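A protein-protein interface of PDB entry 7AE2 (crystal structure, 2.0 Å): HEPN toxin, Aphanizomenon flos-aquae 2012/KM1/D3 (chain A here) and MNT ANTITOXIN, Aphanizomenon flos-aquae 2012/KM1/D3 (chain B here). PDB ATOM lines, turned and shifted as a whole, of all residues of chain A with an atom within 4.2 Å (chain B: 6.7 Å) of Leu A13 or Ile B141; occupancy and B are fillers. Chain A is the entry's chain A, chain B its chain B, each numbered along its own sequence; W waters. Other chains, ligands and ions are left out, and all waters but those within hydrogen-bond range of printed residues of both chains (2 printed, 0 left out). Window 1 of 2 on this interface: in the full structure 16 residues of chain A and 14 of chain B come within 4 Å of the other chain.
Water W2 bridges the side-chain amino group (NZ) of Lys B137 and the side-chain carboxylate (OE2) of Glu A14. Water W1 lies within hydrogen-bond range of the side-chain amide nitrogen (ND2) of Asn A136 (2.7 Å) and the backbone carbonyl oxygen (O) of Leu B138 (2.9 Å).
The side-chain carboxylate (OE1) of Glu A14 lies within salt-bridge range of the side-chain amino group (NZ) of Lys B137. The side-chain carboxylate (OE2) of Glu A14 sits close to the side-chain amide nitrogen (ND2) of Asn B140 (3.5 Å).
Of chain B, only Ile B141 (3.7 Å) comes within 4 Å of Leu A13. Ile B141 touches just these residues of chain A: Glu A10, Leu A13, Val A132 and Asn A136. Of the printed residues of chain B, Val A132 touches Ile B141 and Leu B145. Of the printed residues of chain B, Thr A11 touches Lys B137. Of the printed residues of chain A, Asn B140 touches Glu A14. The nearest printed residue of chain A that does not touch Lys B137 is Glu A10 (4.1 Å).
Printed residues of chain A that touch a printed residue of chain B: Glu A10, Thr A11, Leu A13, Glu A14, Gly A17, Val A132 and Asn A136. Of the 11 printed residues of chain B, 6 touch a printed residue of chain A. Printed residues of chain B that touch a printed residue of chain A: Lys B137, Leu B138, Asn B140, Ile B141, Phe B144 and Leu B145. Hydrophobic or aromatic side chains of chain B within 4 Å of the printed part of chain A: Leu B138, Ile B141, Phe B144 and Leu B145. Along chain B the printed residues that touch a printed residue of chain A span positions 137 to 145. Among the printed residues, 11 pairs touch across the chains.
Among the printed residues, pairs that only touch across the chains: Glu A10 with Leu B138, Glu A10 with Ile B141, Thr A11 with Lys B137, Leu A13 with Ile B141, Gly A17 with Phe B144, Val A132 with Ile B141, Val A132 with Leu B145, Asn A136 with Leu B138 and Asn A136 with Ile B141.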
ATOM      1  N   ILE A   9      13.237  -9.852  -1.243  1.00  0.00           N
ATOM      2  CA  ILE A   9      13.446  -8.461  -1.629  1.00  0.00           C
ATOM      3  C   ILE A   9      12.967  -8.220  -3.056  1.00  0.00           C
ATOM      4  O   ILE A   9      12.350  -7.190  -3.352  1.00  0.00           O
ATOM      5  CB  ILE A   9      14.927  -8.081  -1.450  1.00  0.00           C
ATOM      6  CG1 ILE A   9      15.336  -8.216   0.019  1.00  0.00           C
ATOM      7  CG2 ILE A   9      15.189  -6.667  -1.952  1.00  0.00           C
ATOM      8  CD1 ILE A   9      16.776  -7.848   0.289  1.00  0.00           C
ATOM      9  N   GLU A  10      13.227  -9.170  -3.958  1.00  0.00           N
ATOM     10  CA  GLU A  10      12.807  -9.011  -5.348  1.00  0.00           C
ATOM     11  C   GLU A  10      11.289  -8.934  -5.465  1.00  0.00           C
ATOM     12  O   GLU A  10      10.761  -8.190  -6.301  1.00  0.00           O
ATOM     13  CB  GLU A  10      13.359 -10.158  -6.194  1.00  0.00           C
ATOM     14  CG  GLU A  10      14.857 -10.064  -6.431  1.00  0.00           C
ATOM     15  CD  GLU A  10      15.500 -11.413  -6.685  1.00  0.00           C
ATOM     16  OE1 GLU A  10      14.772 -12.425  -6.734  1.00  0.00           O
ATOM     17  OE2 GLU A  10      16.740 -11.460  -6.833  1.00  0.00           O
ATOM     18  N   THR A  11      10.572  -9.694  -4.632  1.00  0.00           N
ATOM     19  CA  THR A  11       9.114  -9.613  -4.625  1.00  0.00           C
ATOM     20  C   THR A  11       8.641  -8.209  -4.268  1.00  0.00           C
ATOM     21  O   THR A  11       7.712  -7.682  -4.890  1.00  0.00           O
ATOM     22  CB  THR A  11       8.535 -10.636  -3.646  1.00  0.00           C
ATOM     23  OG1 THR A  11       8.915 -11.958  -4.050  1.00  0.00           O
ATOM     24  CG2 THR A  11       7.017 -10.542  -3.607  1.00  0.00           C
ATOM     25  N   ARG A  12       9.273  -7.582  -3.273  1.00  0.00           N
ATOM     26  CA  ARG A  12       8.854  -6.244  -2.869  1.00  0.00           C
ATOM     27  C   ARG A  12       9.265  -5.195  -3.897  1.00  0.00           C
ATOM     28  O   ARG A  12       8.517  -4.245  -4.150  1.00  0.00           O
ATOM     29  CB  ARG A  12       9.427  -5.908  -1.493  1.00  0.00           C
ATOM     30  CG  ARG A  12       8.916  -6.804  -0.379  1.00  0.00           C
ATOM     31  CD  ARG A  12       7.402  -6.728  -0.272  1.00  0.00           C
ATOM     32  NE  ARG A  12       6.892  -7.498   0.859  1.00  0.00           N
ATOM     33  CZ  ARG A  12       5.601  -7.638   1.141  1.00  0.00           C
ATOM     34  NH1 ARG A  12       4.689  -7.061   0.371  1.00  0.00           N
ATOM     35  NH2 ARG A  12       5.222  -8.355   2.190  1.00  0.00           N
ATOM     36  N   LEU A  13      10.452  -5.342  -4.492  1.00  0.00           N
ATOM     37  CA  LEU A  13      10.849  -4.429  -5.561  1.00  0.00           C
ATOM     38  C   LEU A  13       9.891  -4.525  -6.740  1.00  0.00           C
ATOM     39  O   LEU A  13       9.559  -3.512  -7.366  1.00  0.00           O
ATOM     40  CB  LEU A  13      12.277  -4.728  -6.016  1.00  0.00           C
ATOM     41  CG  LEU A  13      13.427  -4.265  -5.126  1.00  0.00           C
ATOM     42  CD1 LEU A  13      14.747  -4.630  -5.786  1.00  0.00           C
ATOM     43  CD2 LEU A  13      13.347  -2.763  -4.875  1.00  0.00           C
ATOM     44  N   GLU A  14       9.440  -5.740  -7.054  1.00  0.00           N
ATOM     45  CA  GLU A  14       8.466  -5.925  -8.122  1.00  0.00           C
ATOM     46  C   GLU A  14       7.164  -5.194  -7.811  1.00  0.00           C
ATOM     47  O   GLU A  14       6.562  -4.578  -8.697  1.00  0.00           O
ATOM     48  CB  GLU A  14       8.216  -7.420  -8.328  1.00  0.00           C
ATOM     49  CG  GLU A  14       7.748  -7.806  -9.716  1.00  0.00           C
ATOM     50  CD  GLU A  14       7.537  -9.303  -9.850  1.00  0.00           C
ATOM     51  OE1 GLU A  14       7.302  -9.961  -8.814  1.00  0.00           O
ATOM     52  OE2 GLU A  14       7.614  -9.819 -10.984  1.00  0.00           O
ATOM     53  N   LEU A  15       6.725  -5.238  -6.550  1.00  0.00           N
ATOM     54  CA  LEU A  15       5.506  -4.533  -6.161  1.00  0.00           C
ATOM     55  C   LEU A  15       5.680  -3.022  -6.256  1.00  0.00           C
ATOM     56  O   LEU A  15       4.766  -2.314  -6.696  1.00  0.00           O
ATOM     57  CB  LEU A  15       5.096  -4.933  -4.745  1.00  0.00           C
ATOM     58  CG  LEU A  15       4.477  -6.321  -4.584  1.00  0.00           C
ATOM     59  CD1 LEU A  15       4.320  -6.669  -3.111  1.00  0.00           C
ATOM     60  CD2 LEU A  15       3.133  -6.385  -5.297  1.00  0.00           C
ATOM     61  N   ILE A  16       6.840  -2.508  -5.834  1.00  0.00           N
ATOM     62  CA  ILE A  16       7.098  -1.072  -5.936  1.00  0.00           C
ATOM     63  C   ILE A  16       7.000  -0.617  -7.386  1.00  0.00           C
ATOM     64  O   ILE A  16       6.424   0.437  -7.685  1.00  0.00           O
ATOM     65  CB  ILE A  16       8.469  -0.729  -5.324  1.00  0.00           C
ATOM     66  CG1 ILE A  16       8.447  -0.951  -3.812  1.00  0.00           C
ATOM     67  CG2 ILE A  16       8.867   0.707  -5.660  1.00  0.00           C
ATOM     68  CD1 ILE A  16       9.777  -0.704  -3.134  1.00  0.00           C
ATOM     69  N   GLY A  17       7.547  -1.412  -8.307  1.00  0.00           N
ATOM     70  CA  GLY A  17       7.450  -1.065  -9.717  1.00  0.00           C
ATOM     71  C   GLY A  17       6.025  -1.029 -10.212  1.00  0.00           C
ATOM     72  O   GLY A  17       5.654  -0.167 -11.019  1.00  0.00           O
ATOM     73  N   ILE A  58      11.854  -3.791   2.838  1.00  0.00           N
ATOM     74  CA  ILE A  58      13.144  -4.164   2.265  1.00  0.00           C
ATOM     75  C   ILE A  58      14.280  -3.714   3.174  1.00  0.00           C
ATOM     76  O   ILE A  58      15.219  -4.474   3.443  1.00  0.00           O
ATOM     77  CB  ILE A  58      13.288  -3.575   0.849  1.00  0.00           C
ATOM     78  CG1 ILE A  58      12.313  -4.255  -0.115  1.00  0.00           C
ATOM     79  CG2 ILE A  58      14.728  -3.698   0.357  1.00  0.00           C
ATOM     80  CD1 ILE A  58      12.302  -3.654  -1.506  1.00  0.00           C
ATOM     81  N   VAL A 132      14.715   1.533  -6.594  1.00  0.00           N
ATOM     82  CA  VAL A 132      14.620   0.201  -7.190  1.00  0.00           C
ATOM     83  C   VAL A 132      15.925  -0.164  -7.888  1.00  0.00           C
ATOM     84  O   VAL A 132      16.407  -1.298  -7.779  1.00  0.00           O
ATOM     85  CB  VAL A 132      13.418   0.128  -8.151  1.00  0.00           C
ATOM     86  CG1 VAL A 132      13.378  -1.222  -8.856  1.00  0.00           C
ATOM     87  CG2 VAL A 132      12.115   0.367  -7.392  1.00  0.00           C
ATOM     88  N   ILE A 135      18.750  -0.904  -5.086  1.00  0.00           N
ATOM     89  CA  ILE A 135      18.547  -2.183  -4.412  1.00  0.00           C
ATOM     90  C   ILE A 135      18.787  -3.334  -5.382  1.00  0.00           C
ATOM     91  O   ILE A 135      19.365  -4.364  -5.016  1.00  0.00           O
ATOM     92  CB  ILE A 135      17.143  -2.250  -3.780  1.00  0.00           C
ATOM     93  CG1 ILE A 135      16.959  -1.123  -2.762  1.00  0.00           C
ATOM     94  CG2 ILE A 135      16.930  -3.594  -3.098  1.00  0.00           C
ATOM     95  CD1 ILE A 135      17.893  -1.212  -1.574  1.00  0.00           C
ATOM     96  N   ASN A 136      18.369  -3.168  -6.641  1.00  0.00           N
ATOM     97  CA  ASN A 136      18.617  -4.196  -7.650  1.00  0.00           C
ATOM     98  C   ASN A 136      20.110  -4.422  -7.858  1.00  0.00           C
ATOM     99  O   ASN A 136      20.557  -5.566  -8.005  1.00  0.00           O
ATOM    100  CB  ASN A 136      17.942  -3.808  -8.966  1.00  0.00           C
ATOM    101  CG  ASN A 136      18.095  -4.872 -10.036  1.00  0.00           C
ATOM    102  OD1 ASN A 136      18.874  -4.716 -10.975  1.00  0.00           O
ATOM    103  ND2 ASN A 136      17.349  -5.960  -9.898  1.00  0.00           N
ATOM    104  N   LEU A 139      21.462  -6.514  -4.997  1.00  0.00           N
ATOM    105  CA  LEU A 139      21.167  -7.938  -5.118  1.00  0.00           C
ATOM    106  C   LEU A 139      22.072  -8.610  -6.143  1.00  0.00           C
ATOM    107  O   LEU A 139      22.474  -9.767  -5.960  1.00  0.00           O
ATOM    108  CB  LEU A 139      19.698  -8.138  -5.490  1.00  0.00           C
ATOM    109  CG  LEU A 139      18.685  -7.666  -4.448  1.00  0.00           C
ATOM    110  CD1 LEU A 139      17.278  -7.782  -4.997  1.00  0.00           C
ATOM    111  CD2 LEU A 139      18.830  -8.467  -3.162  1.00  0.00           C
ATOM    112  N   THR B 136      12.469 -14.748 -12.947  1.00  0.00           N
ATOM    113  CA  THR B 136      11.298 -14.045 -13.461  1.00  0.00           C
ATOM    114  C   THR B 136      11.156 -12.664 -12.830  1.00  0.00           C
ATOM    115  O   THR B 136      10.872 -11.683 -13.527  1.00  0.00           O
ATOM    116  CB  THR B 136      10.037 -14.877 -13.221  1.00  0.00           C
ATOM    117  OG1 THR B 136      10.147 -16.120 -13.922  1.00  0.00           O
ATOM    118  CG2 THR B 136       8.800 -14.132 -13.711  1.00  0.00           C
ATOM    119  N   LYS B 137      11.352 -12.565 -11.515  1.00  0.00           N
ATOM    120  CA  LYS B 137      11.211 -11.272 -10.857  1.00  0.00           C
ATOM    121  C   LYS B 137      12.351 -10.329 -11.221  1.00  0.00           C
ATOM    122  O   LYS B 137      12.131  -9.121 -11.358  1.00  0.00           O
ATOM    123  CB  LYS B 137      11.115 -11.464  -9.345  1.00  0.00           C
ATOM    124  CG  LYS B 137       9.921 -12.313  -8.930  1.00  0.00           C
ATOM    125  CD  LYS B 137       9.704 -12.282  -7.433  1.00  0.00           C
ATOM    126  CE  LYS B 137       8.448 -13.046  -7.048  1.00  0.00           C
ATOM    127  NZ  LYS B 137       7.241 -12.575  -7.791  1.00  0.00           N
ATOM    128  N   LEU B 138      13.565 -10.855 -11.399  1.00  0.00           N
ATOM    129  CA  LEU B 138      14.672 -10.006 -11.829  1.00  0.00           C
ATOM    130  C   LEU B 138      14.437  -9.461 -13.231  1.00  0.00           C
ATOM    131  O   LEU B 138      14.765  -8.303 -13.515  1.00  0.00           O
ATOM    132  CB  LEU B 138      15.988 -10.778 -11.766  1.00  0.00           C
ATOM    133  CG  LEU B 138      16.549 -11.037 -10.369  1.00  0.00           C
ATOM    134  CD1 LEU B 138      17.806 -11.882 -10.467  1.00  0.00           C
ATOM    135  CD2 LEU B 138      16.831  -9.727  -9.644  1.00  0.00           C
ATOM    136  N   GLU B 139      13.872 -10.278 -14.124  1.00  0.00           N
ATOM    137  CA  GLU B 139      13.519  -9.784 -15.451  1.00  0.00           C
ATOM    138  C   GLU B 139      12.429  -8.724 -15.367  1.00  0.00           C
ATOM    139  O   GLU B 139      12.443  -7.743 -16.122  1.00  0.00           O
ATOM    140  CB  GLU B 139      13.072 -10.940 -16.346  1.00  0.00           C
ATOM    141  CG  GLU B 139      14.185 -11.901 -16.727  1.00  0.00           C
ATOM    142  CD  GLU B 139      13.678 -13.114 -17.488  1.00  0.00           C
ATOM    143  OE1 GLU B 139      12.445 -13.282 -17.595  1.00  0.00           O
ATOM    144  OE2 GLU B 139      14.517 -13.899 -17.979  1.00  0.00           O
ATOM    145  N   ASN B 140      11.472  -8.902 -14.454  1.00  0.00           N
ATOM    146  CA  ASN B 140      10.420  -7.907 -14.285  1.00  0.00           C
ATOM    147  C   ASN B 140      10.992  -6.595 -13.762  1.00  0.00           C
ATOM    148  O   ASN B 140      10.606  -5.513 -14.218  1.00  0.00           O
ATOM    149  CB  ASN B 140       9.341  -8.443 -13.343  1.00  0.00           C
ATOM    150  CG  ASN B 140       8.079  -7.599 -13.350  1.00  0.00           C
ATOM    151  OD1 ASN B 140       8.058  -6.491 -12.815  1.00  0.00           O
ATOM    152  ND2 ASN B 140       7.014  -8.129 -13.944  1.00  0.00           N
ATOM    153  N   ILE B 141      11.921  -6.676 -12.807  1.00  0.00           N
ATOM    154  CA  ILE B 141      12.550  -5.474 -12.268  1.00  0.00           C
ATOM    155  C   ILE B 141      13.381  -4.778 -13.340  1.00  0.00           C
ATOM    156  O   ILE B 141      13.320  -3.552 -13.496  1.00  0.00           O
ATOM    157  CB  ILE B 141      13.396  -5.828 -11.031  1.00  0.00           C
ATOM    158  CG1 ILE B 141      12.495  -6.328  -9.898  1.00  0.00           C
ATOM    159  CG2 ILE B 141      14.214  -4.628 -10.569  1.00  0.00           C
ATOM    160  CD1 ILE B 141      13.246  -7.003  -8.769  1.00  0.00           C
ATOM    161  N   GLU B 142      14.162  -5.549 -14.106  1.00  0.00           N
ATOM    162  CA  GLU B 142      14.991  -4.950 -15.149  1.00  0.00           C
ATOM    163  C   GLU B 142      14.137  -4.295 -16.227  1.00  0.00           C
ATOM    164  O   GLU B 142      14.500  -3.239 -16.759  1.00  0.00           O
ATOM    165  CB  GLU B 142      15.917  -6.002 -15.761  1.00  0.00           C
ATOM    166  CG  GLU B 142      16.846  -5.458 -16.839  1.00  0.00           C
ATOM    167  CD  GLU B 142      17.752  -4.347 -16.331  1.00  0.00           C
ATOM    168  OE1 GLU B 142      18.202  -4.428 -15.167  1.00  0.00           O
ATOM    169  OE2 GLU B 142      18.010  -3.390 -17.092  1.00  0.00           O
ATOM    170  N   ASN B 143      12.994  -4.902 -16.558  1.00  0.00           N
ATOM    171  CA  ASN B 143      12.088  -4.290 -17.525  1.00  0.00           C
ATOM    172  C   ASN B 143      11.521  -2.979 -16.998  1.00  0.00           C
ATOM    173  O   ASN B 143      11.385  -2.006 -17.749  1.00  0.00           O
ATOM    174  CB  ASN B 143      10.959  -5.257 -17.876  1.00  0.00           C
ATOM    175  CG  ASN B 143       9.817  -4.575 -18.604  1.00  0.00           C
ATOM    176  OD1 ASN B 143       8.821  -4.186 -17.992  1.00  0.00           O
ATOM    177  ND2 ASN B 143       9.962  -4.413 -19.914  1.00  0.00           N
ATOM    178  N   PHE B 144      11.172  -2.938 -15.709  1.00  0.00           N
ATOM    179  CA  PHE B 144      10.730  -1.690 -15.096  1.00  0.00           C
ATOM    180  C   PHE B 144      11.802  -0.614 -15.217  1.00  0.00           C
ATOM    181  O   PHE B 144      11.514   0.531 -15.584  1.00  0.00           O
ATOM    182  CB  PHE B 144      10.367  -1.929 -13.629  1.00  0.00           C
ATOM    183  CG  PHE B 144      10.226  -0.666 -12.827  1.00  0.00           C
ATOM    184  CD1 PHE B 144       9.020   0.011 -12.786  1.00  0.00           C
ATOM    185  CD2 PHE B 144      11.301  -0.157 -12.112  1.00  0.00           C
ATOM    186  CE1 PHE B 144       8.889   1.178 -12.054  1.00  0.00           C
ATOM    187  CE2 PHE B 144      11.177   1.011 -11.384  1.00  0.00           C
ATOM    188  CZ  PHE B 144       9.970   1.678 -11.355  1.00  0.00           C
ATOM    189  N   LEU B 145      13.052  -0.967 -14.908  1.00  0.00           N
ATOM    190  CA  LEU B 145      14.130   0.017 -14.949  1.00  0.00           C
ATOM    191  C   LEU B 145      14.348   0.542 -16.364  1.00  0.00           C
ATOM    192  O   LEU B 145      14.638   1.729 -16.552  1.00  0.00           O
ATOM    193  CB  LEU B 145      15.414  -0.596 -14.391  1.00  0.00           C
ATOM    194  CG  LEU B 145      15.351  -1.029 -12.925  1.00  0.00           C
ATOM    195  CD1 LEU B 145      16.574  -1.851 -12.559  1.00  0.00           C
ATOM    196  CD2 LEU B 145      15.221   0.183 -12.008  1.00  0.00           C
ATOM    197  N   GLN B 146      14.202  -0.323 -17.371  1.00  0.00           N
ATOM    198  CA  GLN B 146      14.369   0.117 -18.753  1.00  0.00           C
ATOM    199  C   GLN B 146      13.241   1.045 -19.186  1.00  0.00           C
ATOM    200  O   GLN B 146      13.482   2.044 -19.874  1.00  0.00           O
ATOM    201  CB  GLN B 146      14.445  -1.090 -19.688  1.00  0.00           C
ATOM    202  CG  GLN B 146      15.654  -1.976 -19.465  1.00  0.00           C
ATOM    203  CD  GLN B 146      15.697  -3.150 -20.421  1.00  0.00           C
ATOM    204  OE1 GLN B 146      14.948  -3.200 -21.398  1.00  0.00           O
ATOM    205  NE2 GLN B 146      16.575  -4.107 -20.142  1.00  0.00           N
HETATM  206  O   HOH W   1      17.172  -7.165 -12.305  1.00  0.00           O
HETATM  207  O   HOH W   2       6.532 -12.532 -10.390  1.00  0.00           O
